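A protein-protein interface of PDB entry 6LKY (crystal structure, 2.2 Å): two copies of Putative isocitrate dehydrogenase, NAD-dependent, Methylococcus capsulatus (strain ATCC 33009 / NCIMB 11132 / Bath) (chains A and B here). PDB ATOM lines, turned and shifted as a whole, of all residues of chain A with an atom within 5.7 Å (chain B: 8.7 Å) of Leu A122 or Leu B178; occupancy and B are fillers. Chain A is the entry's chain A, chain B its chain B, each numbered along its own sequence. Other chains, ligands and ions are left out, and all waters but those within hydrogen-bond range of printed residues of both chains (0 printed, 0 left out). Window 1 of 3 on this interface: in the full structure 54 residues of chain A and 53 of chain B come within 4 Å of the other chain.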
ATOM      1  N   ARG A  78      20.192  11.445  -1.394  1.00  0.00           N
ATOM      2  CA  ARG A  78      19.897  10.530  -2.486  1.00  0.00           C
ATOM      3  C   ARG A  78      20.622   9.206  -2.262  1.00  0.00           C
ATOM      4  O   ARG A  78      21.689   9.157  -1.642  1.00  0.00           O
ATOM      5  CB  ARG A  78      20.317  11.129  -3.837  1.00  0.00           C
ATOM      6  CG  ARG A  78      19.608  12.422  -4.225  1.00  0.00           C
ATOM      7  CD  ARG A  78      18.392  12.176  -5.135  1.00  0.00           C
ATOM      8  NE  ARG A  78      17.395  13.230  -4.989  1.00  0.00           N
ATOM      9  CZ  ARG A  78      16.127  13.121  -5.376  1.00  0.00           C
ATOM     10  NH1 ARG A  78      15.278  14.126  -5.196  1.00  0.00           N
ATOM     11  NH2 ARG A  78      15.703  12.007  -5.954  1.00  0.00           N
ATOM     12  N   GLU A 120      19.781   5.583 -15.565  1.00  0.00           N
ATOM     13  CA  GLU A 120      18.830   6.656 -15.880  1.00  0.00           C
ATOM     14  C   GLU A 120      17.382   6.224 -15.610  1.00  0.00           C
ATOM     15  O   GLU A 120      17.103   5.623 -14.563  1.00  0.00           O
ATOM     16  CB  GLU A 120      19.035   7.128 -17.333  1.00  0.00           C
ATOM     17  CG  GLU A 120      19.075   5.995 -18.378  1.00  0.00           C
ATOM     18  CD  GLU A 120      19.322   6.481 -19.816  1.00  0.00           C
ATOM     19  OE1 GLU A 120      20.063   7.476 -19.999  1.00  0.00           O
ATOM     20  OE2 GLU A 120      18.794   5.851 -20.771  1.00  0.00           O
ATOM     21  N   GLY A 121      16.448   6.530 -16.518  1.00  0.00           N
ATOM     22  CA  GLY A 121      15.043   6.227 -16.246  1.00  0.00           C
ATOM     23  C   GLY A 121      14.532   7.044 -15.074  1.00  0.00           C
ATOM     24  O   GLY A 121      14.861   8.228 -14.925  1.00  0.00           O
ATOM     25  N   LEU A 122      13.747   6.403 -14.202  1.00  0.00           N
ATOM     26  CA  LEU A 122      13.212   7.109 -13.038  1.00  0.00           C
ATOM     27  C   LEU A 122      14.236   7.270 -11.912  1.00  0.00           C
ATOM     28  O   LEU A 122      13.892   7.797 -10.846  1.00  0.00           O
ATOM     29  CB  LEU A 122      11.961   6.405 -12.507  1.00  0.00           C
ATOM     30  CG  LEU A 122      10.645   6.658 -13.258  1.00  0.00           C
ATOM     31  CD1 LEU A 122       9.663   5.559 -12.986  1.00  0.00           C
ATOM     32  CD2 LEU A 122      10.024   7.989 -12.895  1.00  0.00           C
ATOM     33  N   TYR A 123      15.489   6.873 -12.135  1.00  0.00           N
ATOM     34  CA  TYR A 123      16.553   7.061 -11.157  1.00  0.00           C
ATOM     35  C   TYR A 123      17.446   8.234 -11.510  1.00  0.00           C
ATOM     36  O   TYR A 123      18.481   8.438 -10.866  1.00  0.00           O
ATOM     37  CB  TYR A 123      17.395   5.785 -11.033  1.00  0.00           C
ATOM     38  CG  TYR A 123      16.690   4.667 -10.305  1.00  0.00           C
ATOM     39  CD1 TYR A 123      15.458   4.203 -10.743  1.00  0.00           C
ATOM     40  CD2 TYR A 123      17.272   4.053  -9.200  1.00  0.00           C
ATOM     41  CE1 TYR A 123      14.807   3.171 -10.088  1.00  0.00           C
ATOM     42  CE2 TYR A 123      16.628   3.020  -8.529  1.00  0.00           C
ATOM     43  CZ  TYR A 123      15.391   2.584  -8.982  1.00  0.00           C
ATOM     44  OH  TYR A 123      14.725   1.565  -8.342  1.00  0.00           O
ATOM     45  N   ALA A 124      17.063   9.017 -12.516  1.00  0.00           N
ATOM     46  CA  ALA A 124      17.851  10.169 -12.931  1.00  0.00           C
ATOM     47  C   ALA A 124      18.007  11.210 -11.830  1.00  0.00           C
ATOM     48  O   ALA A 124      18.904  12.050 -11.918  1.00  0.00           O
ATOM     49  CB  ALA A 124      17.212  10.808 -14.163  1.00  0.00           C
ATOM     50  N   GLY A 125      17.163  11.197 -10.802  1.00  0.00           N
ATOM     51  CA  GLY A 125      17.316  12.194  -9.761  1.00  0.00           C
ATOM     52  C   GLY A 125      16.717  13.543 -10.104  1.00  0.00           C
ATOM     53  O   GLY A 125      17.165  14.570  -9.575  1.00  0.00           O
ATOM     54  N   GLU A 127      13.450  15.718  -9.952  1.00  0.00           N
ATOM     55  CA  GLU A 127      12.129  15.856  -9.339  1.00  0.00           C
ATOM     56  C   GLU A 127      11.991  17.233  -8.726  1.00  0.00           C
ATOM     57  O   GLU A 127      12.981  17.875  -8.381  1.00  0.00           O
ATOM     58  CB  GLU A 127      11.869  14.891  -8.191  1.00  0.00           C
ATOM     59  CG  GLU A 127      12.424  13.526  -8.233  1.00  0.00           C
ATOM     60  CD  GLU A 127      12.012  12.789  -6.969  1.00  0.00           C
ATOM     61  OE1 GLU A 127      10.874  12.291  -6.951  1.00  0.00           O
ATOM     62  OE2 GLU A 127      12.801  12.746  -5.995  1.00  0.00           O
ATOM     63  N   SER A 141       8.122  13.989 -10.986  1.00  0.00           N
ATOM     64  CA  SER A 141       9.331  13.194 -11.143  1.00  0.00           C
ATOM     65  C   SER A 141       9.496  12.887 -12.619  1.00  0.00           C
ATOM     66  O   SER A 141       8.524  12.538 -13.297  1.00  0.00           O
ATOM     67  CB  SER A 141       9.262  11.886 -10.340  1.00  0.00           C
ATOM     68  OG  SER A 141       9.214  12.136  -8.942  1.00  0.00           O
ATOM     69  N   ILE A 142      10.717  13.016 -13.116  1.00  0.00           N
ATOM     70  CA  ILE A 142      10.987  12.907 -14.541  1.00  0.00           C
ATOM     71  C   ILE A 142      11.789  11.637 -14.784  1.00  0.00           C
ATOM     72  O   ILE A 142      12.861  11.452 -14.203  1.00  0.00           O
ATOM     73  CB  ILE A 142      11.725  14.155 -15.055  1.00  0.00           C
ATOM     74  CG1 ILE A 142      10.854  15.403 -14.818  1.00  0.00           C
ATOM     75  CG2 ILE A 142      12.120  14.000 -16.536  1.00  0.00           C
ATOM     76  CD1 ILE A 142      11.382  16.657 -15.481  1.00  0.00           C
ATOM     77  N   ALA A 143      11.278  10.760 -15.637  1.00  0.00           N
ATOM     78  CA  ALA A 143      12.067   9.634 -16.130  1.00  0.00           C
ATOM     79  C   ALA A 143      12.826  10.063 -17.382  1.00  0.00           C
ATOM     80  O   ALA A 143      12.267  10.733 -18.252  1.00  0.00           O
ATOM     81  CB  ALA A 143      11.173   8.433 -16.420  1.00  0.00           C
ATOM     82  N   VAL A 144      14.104   9.715 -17.455  1.00  0.00           N
ATOM     83  CA  VAL A 144      14.954  10.090 -18.584  1.00  0.00           C
ATOM     84  C   VAL A 144      15.440   8.829 -19.288  1.00  0.00           C
ATOM     85  O   VAL A 144      16.022   7.942 -18.653  1.00  0.00           O
ATOM     86  CB  VAL A 144      16.151  10.951 -18.138  1.00  0.00           C
ATOM     87  CG1 VAL A 144      17.115  11.160 -19.316  1.00  0.00           C
ATOM     88  CG2 VAL A 144      15.657  12.291 -17.621  1.00  0.00           C
ATOM     89  N   ASN A 227      15.299   0.983 -15.444  1.00  0.00           N
ATOM     90  CA  ASN A 227      15.789   0.968 -14.065  1.00  0.00           C
ATOM     91  C   ASN A 227      14.718   0.495 -13.073  1.00  0.00           C
ATOM     92  O   ASN A 227      14.893  -0.519 -12.381  1.00  0.00           O
ATOM     93  CB  ASN A 227      16.300   2.381 -13.730  1.00  0.00           C
ATOM     94  CG  ASN A 227      17.535   2.380 -12.834  1.00  0.00           C
ATOM     95  OD1 ASN A 227      17.640   1.583 -11.908  1.00  0.00           O
ATOM     96  ND2 ASN A 227      18.484   3.282 -13.120  1.00  0.00           N
ATOM     97  N   LEU A 228      13.589   1.210 -12.992  1.00  0.00           N
ATOM     98  CA  LEU A 228      12.581   0.855 -11.993  1.00  0.00           C
ATOM     99  C   LEU A 228      11.954  -0.508 -12.284  1.00  0.00           C
ATOM    100  O   LEU A 228      11.684  -1.291 -11.360  1.00  0.00           O
ATOM    101  CB  LEU A 228      11.508   1.945 -11.904  1.00  0.00           C
ATOM    102  CG  LEU A 228      10.429   1.711 -10.833  1.00  0.00           C
ATOM    103  CD1 LEU A 228      11.053   1.562  -9.458  1.00  0.00           C
ATOM    104  CD2 LEU A 228       9.392   2.828 -10.807  1.00  0.00           C
ATOM    105  N   GLY B 121      -0.180  10.318 -11.630  1.00  0.00           N
ATOM    106  CA  GLY B 121       1.078   9.575 -11.644  1.00  0.00           C
ATOM    107  C   GLY B 121       1.702   9.573 -13.028  1.00  0.00           C
ATOM    108  O   GLY B 121       1.686  10.577 -13.750  1.00  0.00           O
ATOM    109  N   LEU B 122       2.230   8.419 -13.423  1.00  0.00           N
ATOM    110  CA  LEU B 122       2.857   8.264 -14.730  1.00  0.00           C
ATOM    111  C   LEU B 122       1.840   8.124 -15.845  1.00  0.00           C
ATOM    112  O   LEU B 122       2.241   7.879 -16.984  1.00  0.00           O
ATOM    113  CB  LEU B 122       3.782   7.042 -14.736  1.00  0.00           C
ATOM    114  CG  LEU B 122       5.126   7.327 -14.060  1.00  0.00           C
ATOM    115  CD1 LEU B 122       5.777   6.055 -13.592  1.00  0.00           C
ATOM    116  CD2 LEU B 122       6.038   8.118 -14.999  1.00  0.00           C
ATOM    117  N   SER B 141       9.509  11.497 -19.535  1.00  0.00           N
ATOM    118  CA  SER B 141       8.133  11.265 -19.120  1.00  0.00           C
ATOM    119  C   SER B 141       7.972  11.815 -17.713  1.00  0.00           C
ATOM    120  O   SER B 141       8.845  11.619 -16.864  1.00  0.00           O
ATOM    121  CB  SER B 141       7.789   9.774 -19.133  1.00  0.00           C
ATOM    122  OG  SER B 141       7.808   9.249 -20.441  1.00  0.00           O
ATOM    123  N   ILE B 142       6.871  12.503 -17.456  1.00  0.00           N
ATOM    124  CA  ILE B 142       6.676  13.178 -16.176  1.00  0.00           C
ATOM    125  C   ILE B 142       5.575  12.466 -15.404  1.00  0.00           C
ATOM    126  O   ILE B 142       4.463  12.276 -15.917  1.00  0.00           O
ATOM    127  CB  ILE B 142       6.356  14.662 -16.378  1.00  0.00           C
ATOM    128  CG1 ILE B 142       7.474  15.282 -17.235  1.00  0.00           C
ATOM    129  CG2 ILE B 142       6.219  15.362 -15.039  1.00  0.00           C
ATOM    130  CD1 ILE B 142       7.450  16.785 -17.319  1.00  0.00           C
ATOM    131  N   ALA B 143       5.899  12.030 -14.192  1.00  0.00           N
ATOM    132  CA  ALA B 143       4.906  11.564 -13.237  1.00  0.00           C
ATOM    133  C   ALA B 143       4.407  12.760 -12.425  1.00  0.00           C
ATOM    134  O   ALA B 143       5.212  13.574 -11.965  1.00  0.00           O
ATOM    135  CB  ALA B 143       5.510  10.506 -12.318  1.00  0.00           C
ATOM    136  N   VAL B 144       3.087  12.867 -12.258  1.00  0.00           N
ATOM    137  CA  VAL B 144       2.462  13.961 -11.509  1.00  0.00           C
ATOM    138  C   VAL B 144       1.689  13.396 -10.321  1.00  0.00           C
ATOM    139  O   VAL B 144       0.832  12.527 -10.493  1.00  0.00           O
ATOM    140  CB  VAL B 144       1.514  14.792 -12.387  1.00  0.00           C
ATOM    141  CG1 VAL B 144       0.866  15.897 -11.549  1.00  0.00           C
ATOM    142  CG2 VAL B 144       2.252  15.352 -13.594  1.00  0.00           C
ATOM    143  N   VAL B 145       1.965  13.918  -9.130  1.00  0.00           N
ATOM    144  CA  VAL B 145       1.205  13.629  -7.920  1.00  0.00           C
ATOM    145  C   VAL B 145       0.690  14.943  -7.353  1.00  0.00           C
ATOM    146  O   VAL B 145       1.484  15.850  -7.102  1.00  0.00           O
ATOM    147  CB  VAL B 145       2.083  12.912  -6.874  1.00  0.00           C
ATOM    148  CG1 VAL B 145       1.367  12.871  -5.491  1.00  0.00           C
ATOM    149  CG2 VAL B 145       2.465  11.527  -7.369  1.00  0.00           C
ATOM    150  N   HIS B 173       4.863   2.356  -2.163  1.00  0.00           N
ATOM    151  CA  HIS B 173       5.513   3.561  -2.666  1.00  0.00           C
ATOM    152  C   HIS B 173       6.951   3.245  -3.061  1.00  0.00           C
ATOM    153  O   HIS B 173       7.472   2.166  -2.782  1.00  0.00           O
ATOM    154  CB  HIS B 173       5.500   4.643  -1.587  1.00  0.00           C
ATOM    155  CG  HIS B 173       6.298   4.260  -0.378  1.00  0.00           C
ATOM    156  ND1 HIS B 173       7.657   4.481  -0.281  1.00  0.00           N
ATOM    157  CD2 HIS B 173       5.943   3.591   0.748  1.00  0.00           C
ATOM    158  CE1 HIS B 173       8.095   4.005   0.875  1.00  0.00           C
ATOM    159  NE2 HIS B 173       7.075   3.454   1.514  1.00  0.00           N
ATOM    160  N   LYS B 174       7.614   4.228  -3.654  1.00  0.00           N
ATOM    161  CA  LYS B 174       9.058   4.180  -3.874  1.00  0.00           C
ATOM    162  C   LYS B 174       9.683   5.504  -3.430  1.00  0.00           C
ATOM    163  O   LYS B 174      10.418   6.172  -4.160  1.00  0.00           O
ATOM    164  CB  LYS B 174       9.351   3.844  -5.339  1.00  0.00           C
ATOM    165  CG  LYS B 174      10.821   3.576  -5.671  1.00  0.00           C
ATOM    166  CD  LYS B 174      11.282   2.167  -5.248  1.00  0.00           C
ATOM    167  CE  LYS B 174      12.771   1.984  -5.571  1.00  0.00           C
ATOM    168  NZ  LYS B 174      13.364   0.706  -5.051  1.00  0.00           N
ATOM    169  N   ALA B 175       9.409   5.883  -2.188  1.00  0.00           N
ATOM    170  CA  ALA B 175       9.737   7.224  -1.732  1.00  0.00           C
ATOM    171  C   ALA B 175      11.203   7.385  -1.360  1.00  0.00           C
ATOM    172  O   ALA B 175      11.646   8.515  -1.142  1.00  0.00           O
ATOM    173  CB  ALA B 175       8.842   7.603  -0.543  1.00  0.00           C
ATOM    174  N   ASN B 176      11.973   6.301  -1.301  1.00  0.00           N
ATOM    175  CA  ASN B 176      13.408   6.472  -1.121  1.00  0.00           C
ATOM    176  C   ASN B 176      14.061   7.041  -2.373  1.00  0.00           C
ATOM    177  O   ASN B 176      14.994   7.846  -2.268  1.00  0.00           O
ATOM    178  CB  ASN B 176      14.070   5.146  -0.718  1.00  0.00           C
ATOM    179  CG  ASN B 176      13.711   3.982  -1.644  1.00  0.00           C
ATOM    180  OD1 ASN B 176      12.772   4.054  -2.438  1.00  0.00           O
ATOM    181  ND2 ASN B 176      14.460   2.902  -1.532  1.00  0.00           N
ATOM    182  N   ILE B 177      13.568   6.678  -3.554  1.00  0.00           N
ATOM    183  CA  ILE B 177      14.125   7.158  -4.823  1.00  0.00           C
ATOM    184  C   ILE B 177      13.316   8.323  -5.390  1.00  0.00           C
ATOM    185  O   ILE B 177      13.873   9.318  -5.852  1.00  0.00           O
ATOM    186  CB  ILE B 177      14.197   5.996  -5.832  1.00  0.00           C
ATOM    187  CG1 ILE B 177      15.061   4.854  -5.272  1.00  0.00           C
ATOM    188  CG2 ILE B 177      14.663   6.497  -7.179  1.00  0.00           C
ATOM    189  CD1 ILE B 177      16.526   5.234  -5.065  1.00  0.00           C
ATOM    190  N   LEU B 178      11.998   8.182  -5.414  1.00  0.00           N
ATOM    191  CA  LEU B 178      11.091   9.236  -5.863  1.00  0.00           C
ATOM    192  C   LEU B 178      10.664  10.028  -4.632  1.00  0.00           C
ATOM    193  O   LEU B 178       9.573   9.877  -4.085  1.00  0.00           O
ATOM    194  CB  LEU B 178       9.908   8.625  -6.607  1.00  0.00           C
ATOM    195  CG  LEU B 178      10.348   7.739  -7.800  1.00  0.00           C
ATOM    196  CD1 LEU B 178       9.174   6.997  -8.441  1.00  0.00           C
ATOM    197  CD2 LEU B 178      11.085   8.579  -8.864  1.00  0.00           C
ATOM    198  N   LYS B 179      11.593  10.853  -4.163  1.00  0.00           N
ATOM    199  CA  LYS B 179      11.388  11.541  -2.896  1.00  0.00           C
ATOM    200  C   LYS B 179      10.242  12.542  -2.970  1.00  0.00           C
ATOM    201  O   LYS B 179       9.605  12.821  -1.952  1.00  0.00           O
ATOM    202  CB  LYS B 179      12.686  12.230  -2.463  1.00  0.00           C
ATOM    203  CG  LYS B 179      13.793  11.237  -2.087  1.00  0.00           C
ATOM    204  CD  LYS B 179      15.047  11.958  -1.629  1.00  0.00           C
ATOM    205  CE  LYS B 179      16.200  10.981  -1.402  1.00  0.00           C
ATOM    206  NZ  LYS B 179      15.951  10.052  -0.257  1.00  0.00           N
ATOM    207  N   CYS B 180       9.980  13.115  -4.143  1.00  0.00           N
ATOM    208  CA  CYS B 180       8.952  14.150  -4.252  1.00  0.00           C
ATOM    209  C   CYS B 180       7.561  13.563  -4.487  1.00  0.00           C
ATOM    210  O   CYS B 180       6.636  13.852  -3.731  1.00  0.00           O
ATOM    211  CB  CYS B 180       9.328  15.152  -5.354  1.00  0.00           C
ATOM    212  SG  CYS B 180      10.860  16.120  -4.969  1.00  0.00           S
ATOM    213  N   THR B 181       7.389  12.750  -5.532  1.00  0.00           N
ATOM    214  CA  THR B 181       6.054  12.244  -5.852  1.00  0.00           C
ATOM    215  C   THR B 181       5.642  11.156  -4.872  1.00  0.00           C
ATOM    216  O   THR B 181       4.646  11.290  -4.147  1.00  0.00           O
ATOM    217  CB  THR B 181       6.024  11.700  -7.284  1.00  0.00           C
ATOM    218  OG1 THR B 181       7.185  10.886  -7.493  1.00  0.00           O
ATOM    219  CG2 THR B 181       6.007  12.859  -8.296  1.00  0.00           C
ATOM    220  N   SER B 182       6.404  10.058  -4.848  1.00  0.00           N
ATOM    221  CA  SER B 182       6.131   8.979  -3.908  1.00  0.00           C
ATOM    222  C   SER B 182       6.204   9.471  -2.472  1.00  0.00           C
ATOM    223  O   SER B 182       5.392   9.065  -1.632  1.00  0.00           O
ATOM    224  CB  SER B 182       7.116   7.834  -4.135  1.00  0.00           C
ATOM    225  OG  SER B 182       6.408   6.661  -4.416  1.00  0.00           O
ATOM    226  N   GLY B 183       7.165  10.358  -2.175  1.00  0.00           N
ATOM    227  CA  GLY B 183       7.285  10.893  -0.825  1.00  0.00           C
ATOM    228  C   GLY B 183       6.068  11.691  -0.388  1.00  0.00           C
ATOM    229  O   GLY B 183       5.616  11.578   0.753  1.00  0.00           O
ATOM    230  N   LEU B 184       5.544  12.537  -1.274  1.00  0.00           N
ATOM    231  CA  LEU B 184       4.357  13.304  -0.919  1.00  0.00           C
ATOM    232  C   LEU B 184       3.162  12.382  -0.713  1.00  0.00           C
ATOM    233  O   LEU B 184       2.377  12.565   0.235  1.00  0.00           O
ATOM    234  CB  LEU B 184       4.067  14.345  -1.997  1.00  0.00           C
ATOM    235  CG  LEU B 184       2.838  15.229  -1.798  1.00  0.00           C
ATOM    236  CD1 LEU B 184       2.948  15.989  -0.481  1.00  0.00           C
ATOM    237  CD2 LEU B 184       2.702  16.195  -2.961  1.00  0.00           C
ATOM    238  N   PHE B 185       3.022  11.372  -1.583  1.00  0.00           N
ATOM    239  CA  PHE B 185       1.960  10.376  -1.415  1.00  0.00           C
ATOM    240  C   PHE B 185       2.049   9.691  -0.045  1.00  0.00           C
ATOM    241  O   PHE B 185       1.062   9.627   0.694  1.00  0.00           O
ATOM    242  CB  PHE B 185       2.054   9.360  -2.567  1.00  0.00           C
ATOM    243  CG  PHE B 185       0.910   8.390  -2.636  1.00  0.00           C
ATOM    244  CD1 PHE B 185      -0.342   8.804  -3.018  1.00  0.00           C
ATOM    245  CD2 PHE B 185       1.115   7.038  -2.368  1.00  0.00           C
ATOM    246  CE1 PHE B 185      -1.386   7.903  -3.097  1.00  0.00           C
ATOM    247  CE2 PHE B 185       0.085   6.134  -2.445  1.00  0.00           C
ATOM    248  CZ  PHE B 185      -1.172   6.558  -2.806  1.00  0.00           C
ATOM    249  N   LEU B 186       3.243   9.217   0.323  1.00  0.00           N
ATOM    250  CA  LEU B 186       3.450   8.554   1.618  1.00  0.00           C
ATOM    251  C   LEU B 186       3.168   9.487   2.792  1.00  0.00           C
ATOM    252  O   LEU B 186       2.573   9.075   3.796  1.00  0.00           O
ATOM    253  CB  LEU B 186       4.887   8.031   1.718  1.00  0.00           C
ATOM    254  CG  LEU B 186       5.373   7.447   3.048  1.00  0.00           C
ATOM    255  CD1 LEU B 186       4.536   6.234   3.496  1.00  0.00           C
ATOM    256  CD2 LEU B 186       6.856   7.085   2.923  1.00  0.00           C
ATOM    257  N   ILE B 205       7.949  -0.402   0.419  1.00  0.00           N
ATOM    258  CA  ILE B 205       8.581  -0.042  -0.842  1.00  0.00           C
ATOM    259  C   ILE B 205       8.213  -1.078  -1.901  1.00  0.00           C
ATOM    260  O   ILE B 205       8.206  -2.289  -1.639  1.00  0.00           O
ATOM    261  CB  ILE B 205      10.101   0.087  -0.644  1.00  0.00           C
ATOM    262  CG1 ILE B 205      10.377   1.148   0.441  1.00  0.00           C
ATOM    263  CG2 ILE B 205      10.809   0.481  -1.954  1.00  0.00           C
ATOM    264  CD1 ILE B 205      11.857   1.305   0.840  1.00  0.00           C
ATOM    265  N   VAL B 206       7.902  -0.599  -3.113  1.00  0.00           N
ATOM    266  CA  VAL B 206       7.215  -1.426  -4.106  1.00  0.00           C
ATOM    267  C   VAL B 206       8.001  -2.694  -4.458  1.00  0.00           C
ATOM    268  O   VAL B 206       7.402  -3.748  -4.723  1.00  0.00           O
ATOM    269  CB  VAL B 206       6.881  -0.587  -5.364  1.00  0.00           C
ATOM    270  CG1 VAL B 206       8.141  -0.056  -6.024  1.00  0.00           C
ATOM    271  CG2 VAL B 206       6.061  -1.411  -6.348  1.00  0.00           C
ATOM    272  N   THR B 226      -0.145   4.243  -6.123  1.00  0.00           N
ATOM    273  CA  THR B 226      -0.266   5.110  -7.276  1.00  0.00           C
ATOM    274  C   THR B 226      -0.501   4.277  -8.542  1.00  0.00           C
ATOM    275  O   THR B 226      -0.515   3.041  -8.521  1.00  0.00           O
ATOM    276  CB  THR B 226       0.970   6.009  -7.399  1.00  0.00           C
ATOM    277  OG1 THR B 226       2.165   5.231  -7.246  1.00  0.00           O
ATOM    278  CG2 THR B 226       0.944   7.104  -6.325  1.00  0.00           C
ATOM    279  N   LEU B 228       0.843   3.477 -11.747  1.00  0.00           N
ATOM    280  CA  LEU B 228       1.635   2.410 -12.360  1.00  0.00           C
ATOM    281  C   LEU B 228       1.848   1.250 -11.387  1.00  0.00           C
ATOM    282  O   LEU B 228       1.729   0.070 -11.771  1.00  0.00           O
ATOM    283  CB  LEU B 228       2.993   2.944 -12.832  1.00  0.00           C
ATOM    284  CG  LEU B 228       3.926   1.932 -13.527  1.00  0.00           C
ATOM    285  CD1 LEU B 228       3.194   1.142 -14.605  1.00  0.00           C
ATOM    286  CD2 LEU B 228       5.173   2.566 -14.101  1.00  0.00           C
ATOM    287  N   PHE B 229       2.183   1.566 -10.124  1.00  0.00           N
ATOM    288  CA  PHE B 229       2.411   0.508  -9.145  1.00  0.00           C
ATOM    289  C   PHE B 229       1.142  -0.304  -8.954  1.00  0.00           C
ATOM    290  O   PHE B 229       1.198  -1.527  -8.774  1.00  0.00           O
ATOM    291  CB  PHE B 229       2.878   1.084  -7.800  1.00  0.00           C
ATOM    292  CG  PHE B 229       4.239   1.763  -7.841  1.00  0.00           C
ATOM    293  CD1 PHE B 229       5.111   1.576  -8.913  1.00  0.00           C
ATOM    294  CD2 PHE B 229       4.640   2.596  -6.799  1.00  0.00           C
ATOM    295  CE1 PHE B 229       6.360   2.212  -8.954  1.00  0.00           C
ATOM    296  CE2 PHE B 229       5.893   3.235  -6.823  1.00  0.00           C
ATOM    297  CZ  PHE B 229       6.754   3.042  -7.906  1.00  0.00           C
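Of the 14 printed residues of chain A, 8 touch a printed residue of chain B.
Hydrophobic or aromatic side chains of chain A that line the printed part of chain B: Leu A122, Tyr A123, Ala A143 and Leu A228.
Of the 26 printed residues of chain B, 11 touch a printed residue of chain A.
Hydrophobic or aromatic side chains of chain B that line the printed part of chain A: Leu B122, Ala B143, Ile B177, Leu B178 and Phe B229.
Along chain B the printed residues that touch a printed residue of chain A span positions 122 to 229.
Leu A122 touches three residues of chain B.
Gly A121 touches none of the printed residues of chain B.
Printed residues of chain B within 4 Å of Arg A78: Ile B177 (3.3 Å) and Lys B179 (3.9 Å).
Of the printed residues of chain A, Ile B142 touches Ser A141.
Printed residues of chain B within 4 Å of Tyr A123: Lys B174.
Printed residues of chain B within 4 Å of Leu A228: Phe B229 (3.6 Å).
Of the printed residues of chain A, Ala B143 touches Ser A141.
Gly B183 touches none of the printed residues of chain A.
The nearest printed residue of chain A that does not touch Leu B178 is Ser A141 (4.02 Å).
The nearest printed residue of chain B that does not touch Leu A228 is Lys B174 (4.3 Å).
Leu A122 touches its own counterpart, Leu B122.
Ser B141 touches its own counterpart, Ser A141.
Ser A141 touches Ile B142, and with the chains exchanged Ile A142 touches Ser B141.
Ser A141 touches Ala B143, and with the chains exchanged Ala A143 touches Ser B141.
7 positions are printed for both chains.
Of the 18 pairs that touch across the chains among the printed residues, 6 have their exchanged pair printed and touching as well.
Among the printed residues, pairs that only touch across the chains: Glu A127 with Leu B178, Ile A142 with Ser B141, Tyr A123 with Lys B174, Ser A141 with Ile B142, Leu A122 with Leu B178, Glu A127 with Ile B177, Leu A228 with Phe B229, Ser A141 with Ser B141, Glu A127 with Thr B181, Arg A78 with Lys B179, Leu A122 with Leu B122 and Leu A122 with Ile B177.
The backbone NH of Gly B183 is in hydrogen-bond range of the backbone carbonyl oxygen of Leu B178.
O of Asn B176 lies within hydrogen-bond range of NZ of Lys B179 (3.1 Å).
The side-chain hydroxyl of Ser A141 is in hydrogen-bond range of the side-chain carboxylate of Glu A127, at 2.6 Å.
The guanidinium group (NH1) of Arg A78 is in salt-bridge range of the side-chain carboxylate (OE2) of Glu A127 (2.9 Å).
N of Lys B174 lies within hydrogen-bond range of OG of Ser B182 (2.8 Å).
O of Ser A141 lies within hydrogen-bond range of N of Ala B143 (2.8 Å).
OG of Ser A141 lies within hydrogen-bond range of OG1 of Thr B181 (2.8 Å).
The side-chain carboxylate of Glu A127 is in hydrogen-bond range of the backbone NH of Cys B180 (3.1 Å).
The guanidinium group of Arg A78 sits at hydrogen-bond distance from the backbone carbonyl oxygen of Ile B177.
The backbone NH (N) of Ala A143 lies within hydrogen-bond range of the backbone carbonyl oxygen (O) of Ser B141, 2.9 Å away.
The side-chain carboxylate (OE2) of Glu A127 sits at hydrogen-bond distance from the backbone NH (N) of Lys B179 (2.9 Å).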
